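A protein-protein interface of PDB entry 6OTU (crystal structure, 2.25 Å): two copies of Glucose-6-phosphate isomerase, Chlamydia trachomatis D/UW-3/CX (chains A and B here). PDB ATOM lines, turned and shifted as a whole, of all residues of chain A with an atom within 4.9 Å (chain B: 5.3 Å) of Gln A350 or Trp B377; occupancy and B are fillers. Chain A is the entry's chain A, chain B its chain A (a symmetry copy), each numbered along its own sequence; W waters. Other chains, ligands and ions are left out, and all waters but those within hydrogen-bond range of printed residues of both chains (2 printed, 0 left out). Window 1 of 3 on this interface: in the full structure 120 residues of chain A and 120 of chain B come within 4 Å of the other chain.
The backbone carbonyl oxygen (O) of Trp B377 sits at hydrogen-bond distance from the backbone NH (N) of Val B335. The backbone carbonyl oxygen (O) of Ile B375 lies within hydrogen-bond range of the backbone NH (N) of Thr B333 (2.9 Å). The backbone NH (N) of Trp B377 lies within hydrogen-bond range of the backbone carbonyl oxygen (O) of Thr B333 (3.2 Å). The side-chain sulfur (SD) of Met A354 is in hydrogen-bond range of the backbone NH (N) of Ile A376 (3.4 Å). The side-chain amide nitrogen (NE2) of Gln B350 sits at hydrogen-bond distance from the backbone carbonyl oxygen (O) of Ile B376. NE2 of Gln A350 is in hydrogen-bond range of O of Ile A376 (2.7 Å).
Gln A350 touches Trp B377. Gln A350 touches Phe B388. Met A354 touches Trp B377 (CE to CH2, 3.7 Å). Met A354 touches Phe B388. Ile A375 touches Trp B377. Val B399 touches Ile A375. Trp A377 touches Gln B350. Ile B375 touches Trp A377 (CG2 to CE2, 3.4 Å).
His A348 touches none of the printed residues of chain B. Gln A350 touches just these residues of chain B: Trp B377 (3.3 Å) and Phe B388 (3.4 Å). Printed residues of chain B within 4 Å of Trp A377: Gln B350 (3.3 Å) and Ile B375 (3.4 Å). Of the printed residues of chain A, Gln B350 touches Trp A377 (3.3 Å). Printed residues of chain A within 4 Å of Val B399: Ile A375. The nearest residue of chain A that does not touch Trp B377 is Trp A377 (4.04 Å). The nearest printed residue of chain B that does not touch Trp A377 is Trp B377 (4.04 Å).
Of the 14 printed residues of chain B, 5 touch a printed residue of chain A. Printed residues of chain B that touch a printed residue of chain A: Gln B350, Ile B375, Trp B377, Phe B388 and Val B399. Hydrophobic or aromatic side chains of chain B that line the printed part of chain A: Ile B375, Trp B377, Phe B388 and Val B399. Hydrophobic or aromatic side chains of chain A that line the printed part of chain B: Met A354, Ile A375 and Trp A377. Among the printed residues, no Asp or Glu carboxylate lies within 4 Å of a Lys or Arg side-chain nitrogen of the other chain.
Gln A350 touches Trp B377, and with the chains exchanged Trp A377 touches Gln B350. Ile A375 touches Trp B377, and with the chains exchanged Trp A377 touches Ile B375. 5 positions are printed for both chains. Of the 8 pairs that touch across the chains among the printed residues, 4 have their exchanged pair printed and touching as well.
Water W1 lies within hydrogen-bond range of OD2 of Asp B379 (2.6 Å) and OE1 of Gln A350 (3.0 Å). Water W2 bridges the side-chain amide nitrogen of Gln A350 and the backbone NH of Gly B378.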
ATOM      1  N   THR A 346      12.376  24.662 -17.278  1.00  0.00           N
ATOM      2  CA  THR A 346      12.422  24.885 -18.725  1.00  0.00           C
ATOM      3  C   THR A 346      11.565  26.081 -19.143  1.00  0.00           C
ATOM      4  O   THR A 346      11.929  26.827 -20.062  1.00  0.00           O
ATOM      5  CB  THR A 346      11.971  23.621 -19.463  1.00  0.00           C
ATOM      6  OG1 THR A 346      12.902  22.560 -19.213  1.00  0.00           O
ATOM      7  CG2 THR A 346      11.905  23.856 -20.964  1.00  0.00           C
ATOM      8  N   ALA A 347      10.420  26.278 -18.491  1.00  0.00           N
ATOM      9  CA  ALA A 347       9.593  27.432 -18.815  1.00  0.00           C
ATOM     10  C   ALA A 347      10.347  28.727 -18.551  1.00  0.00           C
ATOM     11  O   ALA A 347      10.299  29.661 -19.361  1.00  0.00           O
ATOM     12  CB  ALA A 347       8.290  27.391 -18.015  1.00  0.00           C
ATOM     13  N   HIS A 348      11.091  28.781 -17.442  1.00  0.00           N
ATOM     14  CA  HIS A 348      11.886  29.964 -17.142  1.00  0.00           C
ATOM     15  C   HIS A 348      13.054  30.132 -18.109  1.00  0.00           C
ATOM     16  O   HIS A 348      13.355  31.253 -18.536  1.00  0.00           O
ATOM     17  CB  HIS A 348      12.422  29.904 -15.722  1.00  0.00           C
ATOM     18  CG  HIS A 348      13.528  30.878 -15.488  1.00  0.00           C
ATOM     19  ND1 HIS A 348      13.338  32.243 -15.568  1.00  0.00           N
ATOM     20  CD2 HIS A 348      14.845  30.693 -15.220  1.00  0.00           C
ATOM     21  CE1 HIS A 348      14.486  32.857 -15.340  1.00  0.00           C
ATOM     22  NE2 HIS A 348      15.415  31.940 -15.123  1.00  0.00           N
ATOM     23  N   LEU A 349      13.757  29.041 -18.422  1.00  0.00           N
ATOM     24  CA  LEU A 349      14.841  29.121 -19.397  1.00  0.00           C
ATOM     25  C   LEU A 349      14.321  29.625 -20.736  1.00  0.00           C
ATOM     26  O   LEU A 349      14.972  30.436 -21.409  1.00  0.00           O
ATOM     27  CB  LEU A 349      15.489  27.749 -19.572  1.00  0.00           C
ATOM     28  CG  LEU A 349      16.168  27.140 -18.352  1.00  0.00           C
ATOM     29  CD1 LEU A 349      16.782  25.782 -18.684  1.00  0.00           C
ATOM     30  CD2 LEU A 349      17.224  28.115 -17.846  1.00  0.00           C
ATOM     31  N   GLN A 350      13.152  29.129 -21.145  1.00  0.00           N
ATOM     32  CA  GLN A 350      12.553  29.551 -22.403  1.00  0.00           C
ATOM     33  C   GLN A 350      12.356  31.066 -22.441  1.00  0.00           C
ATOM     34  O   GLN A 350      12.626  31.708 -23.465  1.00  0.00           O
ATOM     35  CB  GLN A 350      11.236  28.800 -22.590  1.00  0.00           C
ATOM     36  CG  GLN A 350      10.369  29.218 -23.743  1.00  0.00           C
ATOM     37  CD  GLN A 350       9.073  28.425 -23.725  1.00  0.00           C
ATOM     38  OE1 GLN A 350       8.205  28.689 -22.899  1.00  0.00           O
ATOM     39  NE2 GLN A 350       8.961  27.412 -24.591  1.00  0.00           N
ATOM     40  N   GLN A 351      11.909  31.665 -21.329  1.00  0.00           N
ATOM     41  CA  GLN A 351      11.817  33.123 -21.283  1.00  0.00           C
ATOM     42  C   GLN A 351      13.201  33.760 -21.325  1.00  0.00           C
ATOM     43  O   GLN A 351      13.445  34.715 -22.073  1.00  0.00           O
ATOM     44  CB  GLN A 351      11.082  33.590 -20.029  1.00  0.00           C
ATOM     45  CG  GLN A 351      11.356  35.076 -19.760  1.00  0.00           C
ATOM     46  CD  GLN A 351      10.499  35.680 -18.673  1.00  0.00           C
ATOM     47  OE1 GLN A 351      10.257  35.054 -17.643  1.00  0.00           O
ATOM     48  NE2 GLN A 351      10.033  36.913 -18.897  1.00  0.00           N
ATOM     49  N   CYS A 352      14.127  33.227 -20.532  1.00  0.00           N
ATOM     50  CA  CYS A 352      15.392  33.912 -20.336  1.00  0.00           C
ATOM     51  C   CYS A 352      16.214  33.905 -21.618  1.00  0.00           C
ATOM     52  O   CYS A 352      16.808  34.923 -21.991  1.00  0.00           O
ATOM     53  CB  CYS A 352      16.136  33.265 -19.172  1.00  0.00           C
ATOM     54  SG  CYS A 352      17.729  34.089 -18.765  1.00  0.00           S
ATOM     55  N   GLY A 353      16.205  32.785 -22.340  1.00  0.00           N
ATOM     56  CA  GLY A 353      16.921  32.666 -23.599  1.00  0.00           C
ATOM     57  C   GLY A 353      16.230  33.328 -24.774  1.00  0.00           C
ATOM     58  O   GLY A 353      16.870  34.075 -25.513  1.00  0.00           O
ATOM     59  N   MET A 354      14.929  33.078 -24.960  1.00  0.00           N
ATOM     60  CA  MET A 354      14.234  33.618 -26.131  1.00  0.00           C
ATOM     61  C   MET A 354      13.944  35.109 -25.991  1.00  0.00           C
ATOM     62  O   MET A 354      13.957  35.842 -26.989  1.00  0.00           O
ATOM     63  CB  MET A 354      12.939  32.852 -26.381  1.00  0.00           C
ATOM     64  CG  MET A 354      13.190  31.377 -26.687  1.00  0.00           C
ATOM     65  SD  MET A 354      11.703  30.477 -27.130  1.00  0.00           S
ATOM     66  CE  MET A 354      11.390  31.155 -28.746  1.00  0.00           C
ATOM     67  N   GLU A 355      13.637  35.581 -24.781  1.00  0.00           N
ATOM     68  CA  GLU A 355      13.437  37.019 -24.622  1.00  0.00           C
ATOM     69  C   GLU A 355      14.759  37.782 -24.728  1.00  0.00           C
ATOM     70  O   GLU A 355      14.801  38.894 -25.275  1.00  0.00           O
ATOM     71  CB  GLU A 355      12.746  37.319 -23.294  1.00  0.00           C
ATOM     72  CG  GLU A 355      11.958  38.602 -23.317  1.00  0.00           C
ATOM     73  CD  GLU A 355      11.602  39.069 -21.946  1.00  0.00           C
ATOM     74  OE1 GLU A 355      11.061  40.179 -21.838  1.00  0.00           O
ATOM     75  OE2 GLU A 355      11.866  38.334 -20.972  1.00  0.00           O
ATOM     76  N   ILE A 375      14.286  28.257 -30.650  1.00  0.00           N
ATOM     77  CA  ILE A 375      13.160  27.933 -29.784  1.00  0.00           C
ATOM     78  C   ILE A 375      13.678  27.085 -28.634  1.00  0.00           C
ATOM     79  O   ILE A 375      14.403  26.102 -28.838  1.00  0.00           O
ATOM     80  CB  ILE A 375      12.051  27.201 -30.552  1.00  0.00           C
ATOM     81  CG1 ILE A 375      11.726  27.898 -31.875  1.00  0.00           C
ATOM     82  CG2 ILE A 375      10.790  27.093 -29.700  1.00  0.00           C
ATOM     83  CD1 ILE A 375      11.267  29.283 -31.716  1.00  0.00           C
ATOM     84  N   ILE A 376      13.352  27.483 -27.418  1.00  0.00           N
ATOM     85  CA  ILE A 376      13.716  26.708 -26.243  1.00  0.00           C
ATOM     86  C   ILE A 376      12.434  26.073 -25.732  1.00  0.00           C
ATOM     87  O   ILE A 376      11.433  26.764 -25.526  1.00  0.00           O
ATOM     88  CB  ILE A 376      14.420  27.573 -25.187  1.00  0.00           C
ATOM     89  CG1 ILE A 376      15.754  28.079 -25.757  1.00  0.00           C
ATOM     90  CG2 ILE A 376      14.665  26.779 -23.903  1.00  0.00           C
ATOM     91  CD1 ILE A 376      16.451  29.150 -24.909  1.00  0.00           C
ATOM     92  N   TRP A 377      12.445  24.749 -25.609  1.00  0.00           N
ATOM     93  CA  TRP A 377      11.276  23.984 -25.209  1.00  0.00           C
ATOM     94  C   TRP A 377      11.763  22.721 -24.511  1.00  0.00           C
ATOM     95  O   TRP A 377      12.959  22.441 -24.470  1.00  0.00           O
ATOM     96  CB  TRP A 377      10.408  23.659 -26.424  1.00  0.00           C
ATOM     97  CG  TRP A 377      11.081  22.751 -27.385  1.00  0.00           C
ATOM     98  CD1 TRP A 377      12.177  23.030 -28.166  1.00  0.00           C
ATOM     99  CD2 TRP A 377      10.733  21.390 -27.649  1.00  0.00           C
ATOM    100  NE1 TRP A 377      12.520  21.918 -28.916  1.00  0.00           N
ATOM    101  CE2 TRP A 377      11.645  20.903 -28.620  1.00  0.00           C
ATOM    102  CE3 TRP A 377       9.737  20.533 -27.164  1.00  0.00           C
ATOM    103  CZ2 TRP A 377      11.586  19.597 -29.112  1.00  0.00           C
ATOM    104  CZ3 TRP A 377       9.672  19.231 -27.663  1.00  0.00           C
ATOM    105  CH2 TRP A 377      10.593  18.779 -28.628  1.00  0.00           C
ATOM    106  N   THR B 332       8.113  24.731 -36.556  1.00  0.00           N
ATOM    107  CA  THR B 332       7.419  24.630 -35.276  1.00  0.00           C
ATOM    108  C   THR B 332       6.031  25.244 -35.384  1.00  0.00           C
ATOM    109  O   THR B 332       5.704  25.910 -36.364  1.00  0.00           O
ATOM    110  CB  THR B 332       8.169  25.313 -34.107  1.00  0.00           C
ATOM    111  OG1 THR B 332       7.961  26.737 -34.141  1.00  0.00           O
ATOM    112  CG2 THR B 332       9.661  24.996 -34.113  1.00  0.00           C
ATOM    113  N   THR B 333       5.215  24.980 -34.354  1.00  0.00           N
ATOM    114  CA  THR B 333       3.921  25.611 -34.117  1.00  0.00           C
ATOM    115  C   THR B 333       3.796  25.860 -32.622  1.00  0.00           C
ATOM    116  O   THR B 333       3.976  24.932 -31.826  1.00  0.00           O
ATOM    117  CB  THR B 333       2.729  24.739 -34.574  1.00  0.00           C
ATOM    118  OG1 THR B 333       2.871  24.383 -35.948  1.00  0.00           O
ATOM    119  CG2 THR B 333       1.427  25.509 -34.427  1.00  0.00           C
ATOM    120  N   ALA B 334       3.461  27.097 -32.254  1.00  0.00           N
ATOM    121  CA  ALA B 334       3.162  27.475 -30.875  1.00  0.00           C
ATOM    122  C   ALA B 334       1.654  27.482 -30.650  1.00  0.00           C
ATOM    123  O   ALA B 334       0.917  28.202 -31.343  1.00  0.00           O
ATOM    124  CB  ALA B 334       3.732  28.854 -30.546  1.00  0.00           C
ATOM    125  N   VAL B 335       1.201  26.719 -29.667  1.00  0.00           N
ATOM    126  CA  VAL B 335      -0.195  26.725 -29.245  1.00  0.00           C
ATOM    127  C   VAL B 335      -0.306  27.623 -28.015  1.00  0.00           C
ATOM    128  O   VAL B 335       0.341  27.368 -26.994  1.00  0.00           O
ATOM    129  CB  VAL B 335      -0.702  25.300 -28.957  1.00  0.00           C
ATOM    130  CG1 VAL B 335      -2.205  25.296 -28.768  1.00  0.00           C
ATOM    131  CG2 VAL B 335      -0.296  24.333 -30.097  1.00  0.00           C
ATOM    132  N   THR B 346      -1.338  22.336 -23.799  1.00  0.00           N
ATOM    133  CA  THR B 346      -0.259  22.321 -24.790  1.00  0.00           C
ATOM    134  C   THR B 346       0.691  21.142 -24.577  1.00  0.00           C
ATOM    135  O   THR B 346       1.197  20.556 -25.543  1.00  0.00           O
ATOM    136  CB  THR B 346       0.511  23.644 -24.745  1.00  0.00           C
ATOM    137  OG1 THR B 346      -0.353  24.717 -25.141  1.00  0.00           O
ATOM    138  CG2 THR B 346       1.704  23.617 -25.687  1.00  0.00           C
ATOM    139  N   GLN B 350       1.366  18.511 -27.481  1.00  0.00           N
ATOM    140  CA  GLN B 350       2.735  18.231 -27.892  1.00  0.00           C
ATOM    141  C   GLN B 350       2.989  16.727 -27.979  1.00  0.00           C
ATOM    142  O   GLN B 350       3.629  16.252 -28.928  1.00  0.00           O
ATOM    143  CB  GLN B 350       3.687  18.915 -26.912  1.00  0.00           C
ATOM    144  CG  GLN B 350       5.149  18.607 -27.051  1.00  0.00           C
ATOM    145  CD  GLN B 350       5.929  19.304 -25.950  1.00  0.00           C
ATOM    146  OE1 GLN B 350       5.887  18.873 -24.803  1.00  0.00           O
ATOM    147  NE2 GLN B 350       6.592  20.419 -26.277  1.00  0.00           N
ATOM    148  N   ILE B 375       7.757  20.771 -34.296  1.00  0.00           N
ATOM    149  CA  ILE B 375       7.815  20.898 -32.846  1.00  0.00           C
ATOM    150  C   ILE B 375       6.554  21.610 -32.384  1.00  0.00           C
ATOM    151  O   ILE B 375       6.173  22.655 -32.926  1.00  0.00           O
ATOM    152  CB  ILE B 375       9.072  21.657 -32.397  1.00  0.00           C
ATOM    153  CG1 ILE B 375      10.328  21.132 -33.094  1.00  0.00           C
ATOM    154  CG2 ILE B 375       9.242  21.564 -30.884  1.00  0.00           C
ATOM    155  CD1 ILE B 375      10.596  19.712 -32.839  1.00  0.00           C
ATOM    156  N   ILE B 376       5.873  21.026 -31.416  1.00  0.00           N
ATOM    157  CA  ILE B 376       4.698  21.651 -30.831  1.00  0.00           C
ATOM    158  C   ILE B 376       5.106  22.125 -29.446  1.00  0.00           C
ATOM    159  O   ILE B 376       5.647  21.348 -28.654  1.00  0.00           O
ATOM    160  CB  ILE B 376       3.497  20.694 -30.808  1.00  0.00           C
ATOM    161  CG1 ILE B 376       3.091  20.359 -32.252  1.00  0.00           C
ATOM    162  CG2 ILE B 376       2.315  21.315 -30.061  1.00  0.00           C
ATOM    163  CD1 ILE B 376       2.065  19.228 -32.386  1.00  0.00           C
ATOM    164  N   TRP B 377       4.920  23.417 -29.192  1.00  0.00           N
ATOM    165  CA  TRP B 377       5.331  24.041 -27.946  1.00  0.00           C
ATOM    166  C   TRP B 377       4.405  25.223 -27.690  1.00  0.00           C
ATOM    167  O   TRP B 377       3.576  25.571 -28.529  1.00  0.00           O
ATOM    168  CB  TRP B 377       6.793  24.476 -28.021  1.00  0.00           C
ATOM    169  CG  TRP B 377       7.023  25.550 -29.018  1.00  0.00           C
ATOM    170  CD1 TRP B 377       6.917  25.454 -30.385  1.00  0.00           C
ATOM    171  CD2 TRP B 377       7.362  26.909 -28.734  1.00  0.00           C
ATOM    172  NE1 TRP B 377       7.189  26.680 -30.968  1.00  0.00           N
ATOM    173  CE2 TRP B 377       7.471  27.585 -29.977  1.00  0.00           C
ATOM    174  CE3 TRP B 377       7.589  27.625 -27.551  1.00  0.00           C
ATOM    175  CZ2 TRP B 377       7.797  28.941 -30.065  1.00  0.00           C
ATOM    176  CZ3 TRP B 377       7.925  28.977 -27.640  1.00  0.00           C
ATOM    177  CH2 TRP B 377       8.025  29.618 -28.890  1.00  0.00           C
ATOM    178  N   GLY B 378       4.543  25.846 -26.537  1.00  0.00           N
ATOM    179  CA  GLY B 378       3.712  26.993 -26.228  1.00  0.00           C
ATOM    180  C   GLY B 378       3.412  27.085 -24.745  1.00  0.00           C
ATOM    181  O   GLY B 378       3.811  26.240 -23.946  1.00  0.00           O
ATOM    182  N   ASP B 379       2.685  28.147 -24.398  1.00  0.00           N
ATOM    183  CA  ASP B 379       2.258  28.420 -23.031  1.00  0.00           C
ATOM    184  C   ASP B 379       1.108  29.415 -23.098  1.00  0.00           C
ATOM    185  O   ASP B 379       0.703  29.842 -24.184  1.00  0.00           O
ATOM    186  CB  ASP B 379       3.423  28.935 -22.180  1.00  0.00           C
ATOM    187  CG  ASP B 379       3.360  28.443 -20.742  1.00  0.00           C
ATOM    188  OD1 ASP B 379       2.246  28.378 -20.175  1.00  0.00           O
ATOM    189  OD2 ASP B 379       4.428  28.114 -20.176  1.00  0.00           O
ATOM    190  N   PHE B 388       8.564  34.833 -24.319  1.00  0.00           N
ATOM    191  CA  PHE B 388       9.095  34.423 -25.616  1.00  0.00           C
ATOM    192  C   PHE B 388       8.390  35.079 -26.786  1.00  0.00           C
ATOM    193  O   PHE B 388       8.863  34.943 -27.918  1.00  0.00           O
ATOM    194  CB  PHE B 388       9.060  32.893 -25.792  1.00  0.00           C
ATOM    195  CG  PHE B 388       7.708  32.272 -25.621  1.00  0.00           C
ATOM    196  CD1 PHE B 388       6.794  32.253 -26.671  1.00  0.00           C
ATOM    197  CD2 PHE B 388       7.361  31.652 -24.426  1.00  0.00           C
ATOM    198  CE1 PHE B 388       5.549  31.657 -26.520  1.00  0.00           C
ATOM    199  CE2 PHE B 388       6.109  31.064 -24.266  1.00  0.00           C
ATOM    200  CZ  PHE B 388       5.202  31.068 -25.319  1.00  0.00           C
ATOM    201  N   LEU B 392       8.917  35.963 -31.208  1.00  0.00           N
ATOM    202  CA  LEU B 392       7.933  35.944 -32.286  1.00  0.00           C
ATOM    203  C   LEU B 392       7.880  37.293 -32.998  1.00  0.00           C
ATOM    204  O   LEU B 392       7.822  37.345 -34.229  1.00  0.00           O
ATOM    205  CB  LEU B 392       6.558  35.552 -31.737  1.00  0.00           C
ATOM    206  CG  LEU B 392       6.218  34.046 -31.633  1.00  0.00           C
ATOM    207  CD1 LEU B 392       7.193  33.263 -30.821  1.00  0.00           C
ATOM    208  CD2 LEU B 392       4.831  33.837 -31.055  1.00  0.00           C
ATOM    209  N   VAL B 399       7.508  31.763 -36.303  1.00  0.00           N
ATOM    210  CA  VAL B 399       6.798  30.734 -35.549  1.00  0.00           C
ATOM    211  C   VAL B 399       5.301  30.927 -35.764  1.00  0.00           C
ATOM    212  O   VAL B 399       4.726  31.914 -35.281  1.00  0.00           O
ATOM    213  CB  VAL B 399       7.133  30.794 -34.049  1.00  0.00           C
ATOM    214  CG1 VAL B 399       6.335  29.731 -33.301  1.00  0.00           C
ATOM    215  CG2 VAL B 399       8.630  30.631 -33.817  1.00  0.00           C
HETATM  216  O   HOH W   1       6.412  26.874 -21.386  1.00  0.00           O
HETATM  217  O   HOH W   2       6.956  25.090 -24.408  1.00  0.00           O
